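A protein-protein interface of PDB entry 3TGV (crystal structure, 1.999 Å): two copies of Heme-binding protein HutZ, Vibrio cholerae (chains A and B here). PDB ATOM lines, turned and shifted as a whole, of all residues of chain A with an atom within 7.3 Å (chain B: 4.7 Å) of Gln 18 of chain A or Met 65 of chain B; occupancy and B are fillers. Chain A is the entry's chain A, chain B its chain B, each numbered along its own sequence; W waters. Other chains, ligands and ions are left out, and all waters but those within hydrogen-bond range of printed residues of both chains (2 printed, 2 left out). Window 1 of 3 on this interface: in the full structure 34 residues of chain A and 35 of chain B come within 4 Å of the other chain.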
ATOM      1  N   ARG A  14      -6.273 -34.555   9.590  1.00  0.00           N
ATOM      2  CA  ARG A  14      -5.130 -33.977  10.287  1.00  0.00           C
ATOM      3  C   ARG A  14      -4.191 -35.084  10.747  1.00  0.00           C
ATOM      4  O   ARG A  14      -4.629 -36.089  11.297  1.00  0.00           O
ATOM      5  CB  ARG A  14      -5.594 -33.121  11.463  1.00  0.00           C
ATOM      6  CG  ARG A  14      -6.486 -31.951  11.062  1.00  0.00           C
ATOM      7  CD  ARG A  14      -5.672 -30.731  10.664  1.00  0.00           C
ATOM      8  NE  ARG A  14      -5.243 -30.775   9.274  1.00  0.00           N
ATOM      9  CZ  ARG A  14      -4.214 -30.094   8.780  1.00  0.00           C
ATOM     10  NH1 ARG A  14      -3.472 -29.321   9.569  1.00  0.00           N
ATOM     11  NH2 ARG A  14      -3.911 -30.206   7.495  1.00  0.00           N
ATOM     12  N   LYS A  15      -2.896 -34.904  10.507  1.00  0.00           N
ATOM     13  CA  LYS A  15      -1.924 -35.939  10.806  1.00  0.00           C
ATOM     14  C   LYS A  15      -1.039 -35.585  12.001  1.00  0.00           C
ATOM     15  O   LYS A  15      -0.291 -36.428  12.493  1.00  0.00           O
ATOM     16  CB  LYS A  15      -1.056 -36.204   9.570  1.00  0.00           C
ATOM     17  CG  LYS A  15      -1.885 -36.528   8.324  1.00  0.00           C
ATOM     18  CD  LYS A  15      -1.880 -38.020   8.021  1.00  0.00           C
ATOM     19  CE  LYS A  15      -3.126 -38.446   7.259  1.00  0.00           C
ATOM     20  NZ  LYS A  15      -3.325 -37.667   6.007  1.00  0.00           N
ATOM     21  N   THR A  16      -1.122 -34.345  12.464  1.00  0.00           N
ATOM     22  CA  THR A  16      -0.231 -33.869  13.518  1.00  0.00           C
ATOM     23  C   THR A  16      -0.975 -33.221  14.690  1.00  0.00           C
ATOM     24  O   THR A  16      -2.024 -32.587  14.519  1.00  0.00           O
ATOM     25  CB  THR A  16       0.791 -32.846  12.963  1.00  0.00           C
ATOM     26  OG1 THR A  16       1.471 -33.407  11.827  1.00  0.00           O
ATOM     27  CG2 THR A  16       1.818 -32.513  14.013  1.00  0.00           C
ATOM     28  N   LEU A  17      -0.414 -33.402  15.880  1.00  0.00           N
ATOM     29  CA  LEU A  17      -0.845 -32.695  17.073  1.00  0.00           C
ATOM     30  C   LEU A  17       0.167 -31.618  17.421  1.00  0.00           C
ATOM     31  O   LEU A  17       1.392 -31.830  17.314  1.00  0.00           O
ATOM     32  CB  LEU A  17      -0.938 -33.664  18.258  1.00  0.00           C
ATOM     33  CG  LEU A  17      -1.837 -34.892  18.128  1.00  0.00           C
ATOM     34  CD1 LEU A  17      -1.820 -35.730  19.421  1.00  0.00           C
ATOM     35  CD2 LEU A  17      -3.255 -34.448  17.759  1.00  0.00           C
ATOM     36  N   GLN A  18      -0.330 -30.466  17.845  1.00  0.00           N
ATOM     37  CA  GLN A  18       0.529 -29.497  18.504  1.00  0.00           C
ATOM     38  C   GLN A  18       0.409 -29.711  20.004  1.00  0.00           C
ATOM     39  O   GLN A  18      -0.703 -29.885  20.535  1.00  0.00           O
ATOM     40  CB  GLN A  18       0.155 -28.059  18.136  1.00  0.00           C
ATOM     41  CG  GLN A  18      -0.374 -27.883  16.717  1.00  0.00           C
ATOM     42  CD  GLN A  18       0.568 -28.377  15.653  1.00  0.00           C
ATOM     43  OE1 GLN A  18       0.189 -29.159  14.773  1.00  0.00           O
ATOM     44  NE2 GLN A  18       1.806 -27.910  15.708  1.00  0.00           N
ATOM     45  N   LEU A  19       1.548 -29.676  20.691  1.00  0.00           N
ATOM     46  CA  LEU A  19       1.614 -30.031  22.104  1.00  0.00           C
ATOM     47  C   LEU A  19       2.224 -28.931  22.963  1.00  0.00           C
ATOM     48  O   LEU A  19       3.226 -28.325  22.591  1.00  0.00           O
ATOM     49  CB  LEU A  19       2.439 -31.306  22.289  1.00  0.00           C
ATOM     50  CG  LEU A  19       2.169 -32.445  21.315  1.00  0.00           C
ATOM     51  CD1 LEU A  19       3.254 -33.520  21.411  1.00  0.00           C
ATOM     52  CD2 LEU A  19       0.774 -33.026  21.552  1.00  0.00           C
ATOM     53  N   ALA A  20       1.607 -28.683  24.114  1.00  0.00           N
ATOM     54  CA  ALA A  20       2.226 -27.880  25.154  1.00  0.00           C
ATOM     55  C   ALA A  20       2.569 -28.789  26.331  1.00  0.00           C
ATOM     56  O   ALA A  20       1.679 -29.376  26.947  1.00  0.00           O
ATOM     57  CB  ALA A  20       1.310 -26.747  25.590  1.00  0.00           C
ATOM     58  N   VAL A  30       6.442 -25.766  23.594  1.00  0.00           N
ATOM     59  CA  VAL A  30       5.537 -26.073  22.493  1.00  0.00           C
ATOM     60  C   VAL A  30       6.282 -26.859  21.413  1.00  0.00           C
ATOM     61  O   VAL A  30       7.466 -26.610  21.140  1.00  0.00           O
ATOM     62  CB  VAL A  30       4.907 -24.806  21.901  1.00  0.00           C
ATOM     63  CG1 VAL A  30       5.924 -23.990  21.156  1.00  0.00           C
ATOM     64  CG2 VAL A  30       3.722 -25.171  20.988  1.00  0.00           C
ATOM     65  N   SER A  31       5.604 -27.832  20.828  1.00  0.00           N
ATOM     66  CA  SER A  31       6.227 -28.723  19.863  1.00  0.00           C
ATOM     67  C   SER A  31       5.100 -29.323  19.058  1.00  0.00           C
ATOM     68  O   SER A  31       3.935 -28.972  19.270  1.00  0.00           O
ATOM     69  CB  SER A  31       6.969 -29.844  20.591  1.00  0.00           C
ATOM     70  OG  SER A  31       6.064 -30.571  21.408  1.00  0.00           O
ATOM     71  N   TYR A  32       5.432 -30.225  18.138  1.00  0.00           N
ATOM     72  CA  TYR A  32       4.402 -30.987  17.426  1.00  0.00           C
ATOM     73  C   TYR A  32       4.819 -32.459  17.313  1.00  0.00           C
ATOM     74  O   TYR A  32       5.982 -32.805  17.518  1.00  0.00           O
ATOM     75  CB  TYR A  32       4.172 -30.418  16.027  1.00  0.00           C
ATOM     76  CG  TYR A  32       5.202 -30.928  15.050  1.00  0.00           C
ATOM     77  CD1 TYR A  32       6.497 -30.432  15.058  1.00  0.00           C
ATOM     78  CD2 TYR A  32       4.886 -31.929  14.143  1.00  0.00           C
ATOM     79  CE1 TYR A  32       7.467 -30.928  14.176  1.00  0.00           C
ATOM     80  CE2 TYR A  32       5.836 -32.423  13.259  1.00  0.00           C
ATOM     81  CZ  TYR A  32       7.116 -31.916  13.276  1.00  0.00           C
ATOM     82  OH  TYR A  32       8.042 -32.411  12.386  1.00  0.00           O
ATOM     83  N   ALA A  33       3.865 -33.317  16.978  1.00  0.00           N
ATOM     84  CA  ALA A  33       4.159 -34.718  16.709  1.00  0.00           C
ATOM     85  C   ALA A  33       3.071 -35.315  15.826  1.00  0.00           C
ATOM     86  O   ALA A  33       1.883 -35.114  16.082  1.00  0.00           O
ATOM     87  CB  ALA A  33       4.250 -35.492  18.011  1.00  0.00           C
ATOM     88  N   PHE A  35       0.583 -38.202  14.832  1.00  0.00           N
ATOM     89  CA  PHE A  35      -0.128 -39.024  15.807  1.00  0.00           C
ATOM     90  C   PHE A  35      -1.006 -40.050  15.115  1.00  0.00           C
ATOM     91  O   PHE A  35      -1.288 -39.935  13.928  1.00  0.00           O
ATOM     92  CB  PHE A  35      -1.031 -38.146  16.689  1.00  0.00           C
ATOM     93  CG  PHE A  35      -2.280 -37.663  15.985  1.00  0.00           C
ATOM     94  CD1 PHE A  35      -2.214 -36.638  15.048  1.00  0.00           C
ATOM     95  CD2 PHE A  35      -3.520 -38.238  16.256  1.00  0.00           C
ATOM     96  CE1 PHE A  35      -3.361 -36.185  14.406  1.00  0.00           C
ATOM     97  CE2 PHE A  35      -4.671 -37.806  15.607  1.00  0.00           C
ATOM     98  CZ  PHE A  35      -4.603 -36.779  14.694  1.00  0.00           C
ATOM     99  N   VAL A  62      -0.272 -32.642  29.420  1.00  0.00           N
ATOM    100  CA  VAL A  62      -0.100 -32.051  28.106  1.00  0.00           C
ATOM    101  C   VAL A  62      -1.362 -31.302  27.727  1.00  0.00           C
ATOM    102  O   VAL A  62      -2.456 -31.739  28.047  1.00  0.00           O
ATOM    103  CB  VAL A  62       0.010 -33.120  27.024  1.00  0.00           C
ATOM    104  CG1 VAL A  62       0.952 -32.660  25.934  1.00  0.00           C
ATOM    105  CG2 VAL A  62       0.427 -34.430  27.623  1.00  0.00           C
ATOM    106  N   SER A  63      -1.201 -30.196  27.018  1.00  0.00           N
ATOM    107  CA  SER A  63      -2.316 -29.568  26.337  1.00  0.00           C
ATOM    108  C   SER A  63      -2.145 -29.874  24.845  1.00  0.00           C
ATOM    109  O   SER A  63      -1.064 -29.674  24.282  1.00  0.00           O
ATOM    110  CB  SER A  63      -2.362 -28.066  26.640  1.00  0.00           C
ATOM    111  OG  SER A  63      -3.428 -27.410  25.967  1.00  0.00           O
ATOM    112  N   ILE A  64      -3.196 -30.401  24.219  1.00  0.00           N
ATOM    113  CA  ILE A  64      -3.127 -30.874  22.832  1.00  0.00           C
ATOM    114  C   ILE A  64      -4.007 -30.051  21.886  1.00  0.00           C
ATOM    115  O   ILE A  64      -5.132 -29.675  22.232  1.00  0.00           O
ATOM    116  CB  ILE A  64      -3.576 -32.337  22.741  1.00  0.00           C
ATOM    117  CG1 ILE A  64      -2.603 -33.238  23.504  1.00  0.00           C
ATOM    118  CG2 ILE A  64      -3.703 -32.776  21.278  1.00  0.00           C
ATOM    119  CD1 ILE A  64      -3.151 -34.611  23.795  1.00  0.00           C
ATOM    120  N   MET A  65      -3.496 -29.762  20.698  1.00  0.00           N
ATOM    121  CA  MET A  65      -4.282 -29.047  19.695  1.00  0.00           C
ATOM    122  C   MET A  65      -4.104 -29.640  18.304  1.00  0.00           C
ATOM    123  O   MET A  65      -2.981 -29.916  17.860  1.00  0.00           O
ATOM    124  CB  MET A  65      -3.934 -27.556  19.683  1.00  0.00           C
ATOM    125  CG  MET A  65      -4.651 -26.769  18.603  1.00  0.00           C
ATOM    126  SD  MET A  65      -4.412 -24.980  18.727  1.00  0.00           S
ATOM    127  CE  MET A  65      -2.641 -24.887  18.494  1.00  0.00           C
ATOM    128  N   MET A  66      -5.226 -29.841  17.632  1.00  0.00           N
ATOM    129  CA  MET A  66      -5.254 -30.276  16.248  1.00  0.00           C
ATOM    130  C   MET A  66      -5.836 -29.088  15.472  1.00  0.00           C
ATOM    131  O   MET A  66      -6.936 -28.619  15.780  1.00  0.00           O
ATOM    132  CB  MET A  66      -6.148 -31.515  16.156  1.00  0.00           C
ATOM    133  CG  MET A  66      -6.154 -32.270  14.846  1.00  0.00           C
ATOM    134  SD  MET A  66      -7.371 -33.624  14.906  1.00  0.00           S
ATOM    135  CE  MET A  66      -6.869 -34.463  16.393  1.00  0.00           C
ATOM    136  N   ILE A  67      -5.095 -28.572  14.496  1.00  0.00           N
ATOM    137  CA  ILE A  67      -5.450 -27.297  13.869  1.00  0.00           C
ATOM    138  C   ILE A  67      -5.262 -27.261  12.345  1.00  0.00           C
ATOM    139  O   ILE A  67      -4.325 -27.870  11.806  1.00  0.00           O
ATOM    140  CB  ILE A  67      -4.652 -26.130  14.521  1.00  0.00           C
ATOM    141  CG1 ILE A  67      -5.126 -24.787  13.970  1.00  0.00           C
ATOM    142  CG2 ILE A  67      -3.123 -26.331  14.334  1.00  0.00           C
ATOM    143  CD1 ILE A  67      -4.736 -23.617  14.842  1.00  0.00           C
ATOM    144  N   ASP A  69      -4.312 -25.710   8.642  1.00  0.00           N
ATOM    145  CA  ASP A  69      -3.105 -25.000   8.229  1.00  0.00           C
ATOM    146  C   ASP A  69      -3.355 -23.505   8.085  1.00  0.00           C
ATOM    147  O   ASP A  69      -4.469 -23.096   7.786  1.00  0.00           O
ATOM    148  CB  ASP A  69      -2.610 -25.558   6.895  1.00  0.00           C
ATOM    149  CG  ASP A  69      -1.967 -26.926   7.037  1.00  0.00           C
ATOM    150  OD1 ASP A  69      -1.466 -27.231   8.140  1.00  0.00           O
ATOM    151  OD2 ASP A  69      -1.950 -27.687   6.044  1.00  0.00           O
ATOM    152  N   GLU A  70      -2.320 -22.687   8.278  1.00  0.00           N
ATOM    153  CA  GLU A  70      -2.462 -21.258   8.047  1.00  0.00           C
ATOM    154  C   GLU A  70      -3.008 -20.990   6.653  1.00  0.00           C
ATOM    155  O   GLU A  70      -3.922 -20.190   6.491  1.00  0.00           O
ATOM    156  CB  GLU A  70      -1.136 -20.508   8.224  1.00  0.00           C
ATOM    157  CG  GLU A  70      -0.835 -20.115   9.646  1.00  0.00           C
ATOM    158  CD  GLU A  70       0.432 -19.313   9.781  1.00  0.00           C
ATOM    159  OE1 GLU A  70       0.738 -18.510   8.868  1.00  0.00           O
ATOM    160  OE2 GLU A  70       1.143 -19.508  10.792  1.00  0.00           O
ATOM    161  N   ARG A  79      -8.770 -19.995  13.158  1.00  0.00           N
ATOM    162  CA  ARG A  79      -8.351 -21.263  12.582  1.00  0.00           C
ATOM    163  C   ARG A  79      -9.197 -22.396  13.170  1.00  0.00           C
ATOM    164  O   ARG A  79      -9.366 -22.512  14.382  1.00  0.00           O
ATOM    165  CB  ARG A  79      -6.843 -21.495  12.786  1.00  0.00           C
ATOM    166  CG  ARG A  79      -5.948 -20.571  11.945  1.00  0.00           C
ATOM    167  CD  ARG A  79      -4.474 -20.686  12.324  1.00  0.00           C
ATOM    168  NE  ARG A  79      -3.873 -21.923  11.843  1.00  0.00           N
ATOM    169  CZ  ARG A  79      -2.658 -22.350  12.173  1.00  0.00           C
ATOM    170  NH1 ARG A  79      -1.885 -21.643  12.994  1.00  0.00           N
ATOM    171  NH2 ARG A  79      -2.210 -23.490  11.677  1.00  0.00           N
ATOM    172  N   LEU A  82      -9.415 -28.226  17.225  1.00  0.00           N
ATOM    173  CA  LEU A  82      -9.887 -29.023  18.354  1.00  0.00           C
ATOM    174  C   LEU A  82      -8.813 -28.950  19.420  1.00  0.00           C
ATOM    175  O   LEU A  82      -7.641 -29.167  19.122  1.00  0.00           O
ATOM    176  CB  LEU A  82     -10.017 -30.492  17.960  1.00  0.00           C
ATOM    177  CG  LEU A  82     -11.016 -30.907  16.880  1.00  0.00           C
ATOM    178  CD1 LEU A  82     -10.954 -32.399  16.675  1.00  0.00           C
ATOM    179  CD2 LEU A  82     -12.443 -30.462  17.241  1.00  0.00           C
ATOM    180  N   THR A  83      -9.187 -28.666  20.660  1.00  0.00           N
ATOM    181  CA  THR A  83      -8.189 -28.575  21.730  1.00  0.00           C
ATOM    182  C   THR A  83      -8.676 -29.320  22.970  1.00  0.00           C
ATOM    183  O   THR A  83      -9.879 -29.308  23.293  1.00  0.00           O
ATOM    184  CB  THR A  83      -7.884 -27.105  22.089  1.00  0.00           C
ATOM    185  OG1 THR A  83      -7.597 -26.366  20.895  1.00  0.00           O
ATOM    186  CG2 THR A  83      -6.672 -27.014  23.009  1.00  0.00           C
ATOM    187  N   PHE A  84      -7.747 -29.971  23.658  1.00  0.00           N
ATOM    188  CA  PHE A  84      -8.062 -30.688  24.888  1.00  0.00           C
ATOM    189  C   PHE A  84      -6.794 -30.942  25.685  1.00  0.00           C
ATOM    190  O   PHE A  84      -5.700 -30.971  25.120  1.00  0.00           O
ATOM    191  CB  PHE A  84      -8.783 -32.009  24.596  1.00  0.00           C
ATOM    192  CG  PHE A  84      -8.013 -32.961  23.714  1.00  0.00           C
ATOM    193  CD1 PHE A  84      -8.019 -32.812  22.339  1.00  0.00           C
ATOM    194  CD2 PHE A  84      -7.317 -34.034  24.263  1.00  0.00           C
ATOM    195  CE1 PHE A  84      -7.318 -33.692  21.520  1.00  0.00           C
ATOM    196  CE2 PHE A  84      -6.611 -34.926  23.444  1.00  0.00           C
ATOM    197  CZ  PHE A  84      -6.622 -34.751  22.074  1.00  0.00           C
ATOM    198  N   THR B  16       1.227 -16.708  12.036  1.00  0.00           N
ATOM    199  CA  THR B  16       0.864 -17.039  13.413  1.00  0.00           C
ATOM    200  C   THR B  16       1.969 -17.742  14.216  1.00  0.00           C
ATOM    201  O   THR B  16       2.904 -18.353  13.661  1.00  0.00           O
ATOM    202  CB  THR B  16      -0.397 -17.920  13.478  1.00  0.00           C
ATOM    203  OG1 THR B  16      -0.074 -19.241  13.048  1.00  0.00           O
ATOM    204  CG2 THR B  16      -1.511 -17.352  12.589  1.00  0.00           C
ATOM    205  N   LEU B  17       1.845 -17.630  15.532  1.00  0.00           N
ATOM    206  CA  LEU B  17       2.712 -18.321  16.464  1.00  0.00           C
ATOM    207  C   LEU B  17       1.913 -19.394  17.172  1.00  0.00           C
ATOM    208  O   LEU B  17       0.745 -19.186  17.495  1.00  0.00           O
ATOM    209  CB  LEU B  17       3.238 -17.330  17.502  1.00  0.00           C
ATOM    210  CG  LEU B  17       4.009 -16.123  16.966  1.00  0.00           C
ATOM    211  CD1 LEU B  17       4.388 -15.192  18.122  1.00  0.00           C
ATOM    212  CD2 LEU B  17       5.238 -16.583  16.234  1.00  0.00           C
ATOM    213  N   GLN B  18       2.531 -20.543  17.405  1.00  0.00           N
ATOM    214  CA  GLN B  18       1.921 -21.549  18.256  1.00  0.00           C
ATOM    215  C   GLN B  18       2.547 -21.357  19.630  1.00  0.00           C
ATOM    216  O   GLN B  18       3.761 -21.209  19.751  1.00  0.00           O
ATOM    217  CB  GLN B  18       2.195 -22.950  17.719  1.00  0.00           C
ATOM    218  CG  GLN B  18       2.318 -23.016  16.190  1.00  0.00           C
ATOM    219  CD  GLN B  18       1.031 -22.651  15.458  1.00  0.00           C
ATOM    220  OE1 GLN B  18       1.055 -22.040  14.374  1.00  0.00           O
ATOM    221  NE2 GLN B  18      -0.100 -23.040  16.031  1.00  0.00           N
ATOM    222  N   VAL B  30      -2.008 -25.168  25.188  1.00  0.00           N
ATOM    223  CA  VAL B  30      -1.537 -24.927  23.829  1.00  0.00           C
ATOM    224  C   VAL B  30      -2.550 -24.104  23.037  1.00  0.00           C
ATOM    225  O   VAL B  30      -3.767 -24.318  23.138  1.00  0.00           O
ATOM    226  CB  VAL B  30      -1.179 -26.231  23.080  1.00  0.00           C
ATOM    227  CG1 VAL B  30      -2.415 -26.927  22.607  1.00  0.00           C
ATOM    228  CG2 VAL B  30      -0.238 -25.928  21.900  1.00  0.00           C
ATOM    229  N   SER B  63       6.556 -20.635  25.531  1.00  0.00           N
ATOM    230  CA  SER B  63       7.354 -21.250  24.488  1.00  0.00           C
ATOM    231  C   SER B  63       6.634 -20.993  23.180  1.00  0.00           C
ATOM    232  O   SER B  63       5.433 -21.237  23.067  1.00  0.00           O
ATOM    233  CB  SER B  63       7.528 -22.748  24.745  1.00  0.00           C
ATOM    234  OG  SER B  63       8.213 -23.384  23.675  1.00  0.00           O
ATOM    235  N   ILE B  64       7.376 -20.489  22.201  1.00  0.00           N
ATOM    236  CA  ILE B  64       6.807 -20.013  20.952  1.00  0.00           C
ATOM    237  C   ILE B  64       7.330 -20.815  19.779  1.00  0.00           C
ATOM    238  O   ILE B  64       8.519 -21.151  19.725  1.00  0.00           O
ATOM    239  CB  ILE B  64       7.177 -18.548  20.734  1.00  0.00           C
ATOM    240  CG1 ILE B  64       6.570 -17.701  21.857  1.00  0.00           C
ATOM    241  CG2 ILE B  64       6.728 -18.093  19.348  1.00  0.00           C
ATOM    242  CD1 ILE B  64       7.122 -16.294  21.963  1.00  0.00           C
ATOM    243  N   MET B  65       6.451 -21.137  18.841  1.00  0.00           N
ATOM    244  CA  MET B  65       6.889 -21.848  17.643  1.00  0.00           C
ATOM    245  C   MET B  65       6.258 -21.265  16.391  1.00  0.00           C
ATOM    246  O   MET B  65       5.052 -21.023  16.330  1.00  0.00           O
ATOM    247  CB  MET B  65       6.599 -23.355  17.751  1.00  0.00           C
ATOM    248  CG  MET B  65       7.072 -24.170  16.546  1.00  0.00           C
ATOM    249  SD  MET B  65       6.837 -25.966  16.721  1.00  0.00           S
ATOM    250  CE  MET B  65       5.067 -26.092  16.920  1.00  0.00           C
ATOM    251  N   MET B  66       7.093 -21.031  15.389  1.00  0.00           N
ATOM    252  CA  MET B  66       6.620 -20.668  14.073  1.00  0.00           C
ATOM    253  C   MET B  66       6.882 -21.868  13.144  1.00  0.00           C
ATOM    254  O   MET B  66       8.027 -22.285  12.963  1.00  0.00           O
ATOM    255  CB  MET B  66       7.387 -19.429  13.649  1.00  0.00           C
ATOM    256  CG  MET B  66       6.784 -18.623  12.560  1.00  0.00           C
ATOM    257  SD  MET B  66       7.953 -17.351  12.049  1.00  0.00           S
ATOM    258  CE  MET B  66       8.176 -16.476  13.576  1.00  0.00           C
ATOM    259  N   ILE B  67       5.827 -22.439  12.564  1.00  0.00           N
ATOM    260  CA  ILE B  67       5.952 -23.733  11.892  1.00  0.00           C
ATOM    261  C   ILE B  67       5.278 -23.782  10.520  1.00  0.00           C
ATOM    262  O   ILE B  67       4.190 -23.215  10.334  1.00  0.00           O
ATOM    263  CB  ILE B  67       5.384 -24.858  12.793  1.00  0.00           C
ATOM    264  CG1 ILE B  67       5.730 -26.237  12.239  1.00  0.00           C
ATOM    265  CG2 ILE B  67       3.875 -24.703  12.957  1.00  0.00           C
ATOM    266  CD1 ILE B  67       5.412 -27.374  13.199  1.00  0.00           C
ATOM    267  N   ARG B  79       8.946 -31.024  10.190  1.00  0.00           N
ATOM    268  CA  ARG B  79       8.354 -29.787   9.721  1.00  0.00           C
ATOM    269  C   ARG B  79       9.333 -28.650   9.976  1.00  0.00           C
ATOM    270  O   ARG B  79       9.860 -28.510  11.077  1.00  0.00           O
ATOM    271  CB  ARG B  79       6.985 -29.527  10.380  1.00  0.00           C
ATOM    272  CG  ARG B  79       5.882 -30.428   9.827  1.00  0.00           C
ATOM    273  CD  ARG B  79       4.597 -30.369  10.638  1.00  0.00           C
ATOM    274  NE  ARG B  79       3.883 -29.109  10.482  1.00  0.00           N
ATOM    275  CZ  ARG B  79       2.795 -28.786  11.169  1.00  0.00           C
ATOM    276  NH1 ARG B  79       2.283 -29.634  12.052  1.00  0.00           N
ATOM    277  NH2 ARG B  79       2.214 -27.618  10.977  1.00  0.00           N
ATOM    278  N   ARG B  81      10.694 -25.155  10.971  1.00  0.00           N
ATOM    279  CA  ARG B  81      10.160 -24.449  12.134  1.00  0.00           C
ATOM    280  C   ARG B  81      11.200 -23.674  12.922  1.00  0.00           C
ATOM    281  O   ARG B  81      12.381 -24.040  12.939  1.00  0.00           O
ATOM    282  CB  ARG B  81       9.468 -25.453  13.065  1.00  0.00           C
ATOM    283  CG  ARG B  81      10.396 -26.463  13.751  1.00  0.00           C
ATOM    284  CD  ARG B  81       9.610 -27.663  14.328  1.00  0.00           C
ATOM    285  NE  ARG B  81      10.465 -28.594  15.078  1.00  0.00           N
ATOM    286  CZ  ARG B  81      11.129 -29.623  14.543  1.00  0.00           C
ATOM    287  NH1 ARG B  81      11.055 -29.882  13.244  1.00  0.00           N
ATOM    288  NH2 ARG B  81      11.871 -30.403  15.312  1.00  0.00           N
ATOM    289  N   LEU B  82      10.743 -22.616  13.586  1.00  0.00           N
ATOM    290  CA  LEU B  82      11.581 -21.835  14.492  1.00  0.00           C
ATOM    291  C   LEU B  82      10.973 -21.910  15.878  1.00  0.00           C
ATOM    292  O   LEU B  82       9.765 -21.693  16.042  1.00  0.00           O
ATOM    293  CB  LEU B  82      11.623 -20.362  14.062  1.00  0.00           C
ATOM    294  CG  LEU B  82      12.015 -20.020  12.633  1.00  0.00           C
ATOM    295  CD1 LEU B  82      11.925 -18.520  12.395  1.00  0.00           C
ATOM    296  CD2 LEU B  82      13.436 -20.527  12.340  1.00  0.00           C
ATOM    297  N   THR B  83      11.789 -22.196  16.889  1.00  0.00           N
ATOM    298  CA  THR B  83      11.248 -22.236  18.244  1.00  0.00           C
ATOM    299  C   THR B  83      12.088 -21.430  19.215  1.00  0.00           C
ATOM    300  O   THR B  83      13.316 -21.447  19.151  1.00  0.00           O
ATOM    301  CB  THR B  83      11.118 -23.675  18.759  1.00  0.00           C
ATOM    302  OG1 THR B  83      10.425 -24.462  17.783  1.00  0.00           O
ATOM    303  CG2 THR B  83      10.314 -23.699  20.064  1.00  0.00           C
HETATM  304  O   HOH W   1      -6.334 -23.478  22.101  1.00  0.00           O
HETATM  305  O   HOH W   2       0.090 -25.238  12.276  1.00  0.00           O
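Water W1 lies within hydrogen-bond range of the backbone carbonyl oxygen (O) of Val 30 of chain B (2.9 Å) and the side-chain hydroxyl (OG1) of Thr 83 of chain A (3.4 Å). Water W2 lies within hydrogen-bond range of the guanidinium group of Arg 79 of chain A (3.0 Å) and the guanidinium group of Arg 79 of chain B (3.4 Å).
Of the 24 printed residues of chain A, 12 touch a printed residue of chain B. Along chain A the printed residues that touch a printed residue of chain B span positions 16 to 83. Among the printed residues, 21 pairs touch across the chains. Among the printed residues, no Asp or Glu carboxylate lies within 4 Å of a Lys or Arg side-chain nitrogen of the other chain.
OE1 of Gln 18 of chain A lies within hydrogen-bond range of NH1 of Arg 79 of chain B (3.5 Å). N of Val 30 of chain A sits at hydrogen-bond distance from OG of Ser 63 of chain B, 3.0 Å away. N of Arg 79 of chain B lies within hydrogen-bond range of OH of Tyr 32 of chain A. The side-chain hydroxyl (OG) of Ser 63 of chain A is in hydrogen-bond range of the backbone NH (N) of Val 30 of chain B (2.8 Å). The side-chain hydroxyl (OG1) of Thr 16 of chain B sits at hydrogen-bond distance from the side-chain carboxylate (OE2) of Glu 70 of chain A (2.6 Å). The guanidinium group (NH1) of Arg 79 of chain A lies within hydrogen-bond range of the side-chain hydroxyl (OG1) of Thr 16 of chain B (3.0 Å). The guanidinium group (NH1) of Arg 79 of chain A sits at hydrogen-bond distance from the side-chain amide oxygen (OE1) of Gln 18 of chain B (3.3 Å).
Gln 18 of chain A touches Val 30 of chain B. CE of Met 65 of chain B touches NE2 of Gln 18 of chain A (3.9 Å). Ala 20 of chain A touches Val 30 of chain B. Val 30 of chain A touches Gln 18 of chain B. Val 30 of chain A touches Ile 64 of chain B. Met 65 of chain B touches Ser 31 of chain A (CE to C, 3.9 Å). Tyr 32 of chain A touches Ile 67 of chain B. C of Ile 64 of chain A touches CG1 of Val 30 of chain B (3.6 Å).
Of the printed residues of chain B, Gln 18 of chain A touches Val 30, Met 65 and Arg 79. Of chain A, only Gln 18 (3.9 Å), Val 30 (3.5 Å) and Ser 31 (3.9 Å) come within 4 Å of Met 65 of chain B. Printed residues of chain B within 4 Å of Glu 70 of chain A: Thr 16. Printed residues of chain B within 4 Å of Ala 20 of chain A: Val 30 (3.6 Å). Of the printed residues of chain B, Arg 79 of chain A touches Thr 16 (3.0 Å) and Gln 18 (3.3 Å). Leu 17 of chain B touches none of the printed residues of chain A. The nearest printed residue of chain B that does not touch Gln 18 of chain A is Ile 67 of chain B (4.4 Å). The nearest printed residue of chain A that does not touch Ser 63 of chain B is Ser 31 of chain A (5.9 Å).
The backbone NH (N) of Leu 19 of chain A is in hydrogen-bond range of the backbone carbonyl oxygen (O) of Ser 31 of chain A, 2.9 Å away. The backbone carbonyl oxygen of Met 65 of chain B lies within hydrogen-bond range of the backbone NH of Gln 18 of chain B, at 2.8 Å.
Gln 18 of chain A touches Met 65 of chain B, and with the chains exchanged Met 65 of chain A touches Gln 18 of chain B. Val 30 of chain A touches Ser 63 of chain B, and with the chains exchanged Ser 63 of chain A touches Val 30 of chain B. Positions printed for both chains: 16, 17, 18, 30, 63, 64, 65, 66, 67, 79, 82 and 83.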
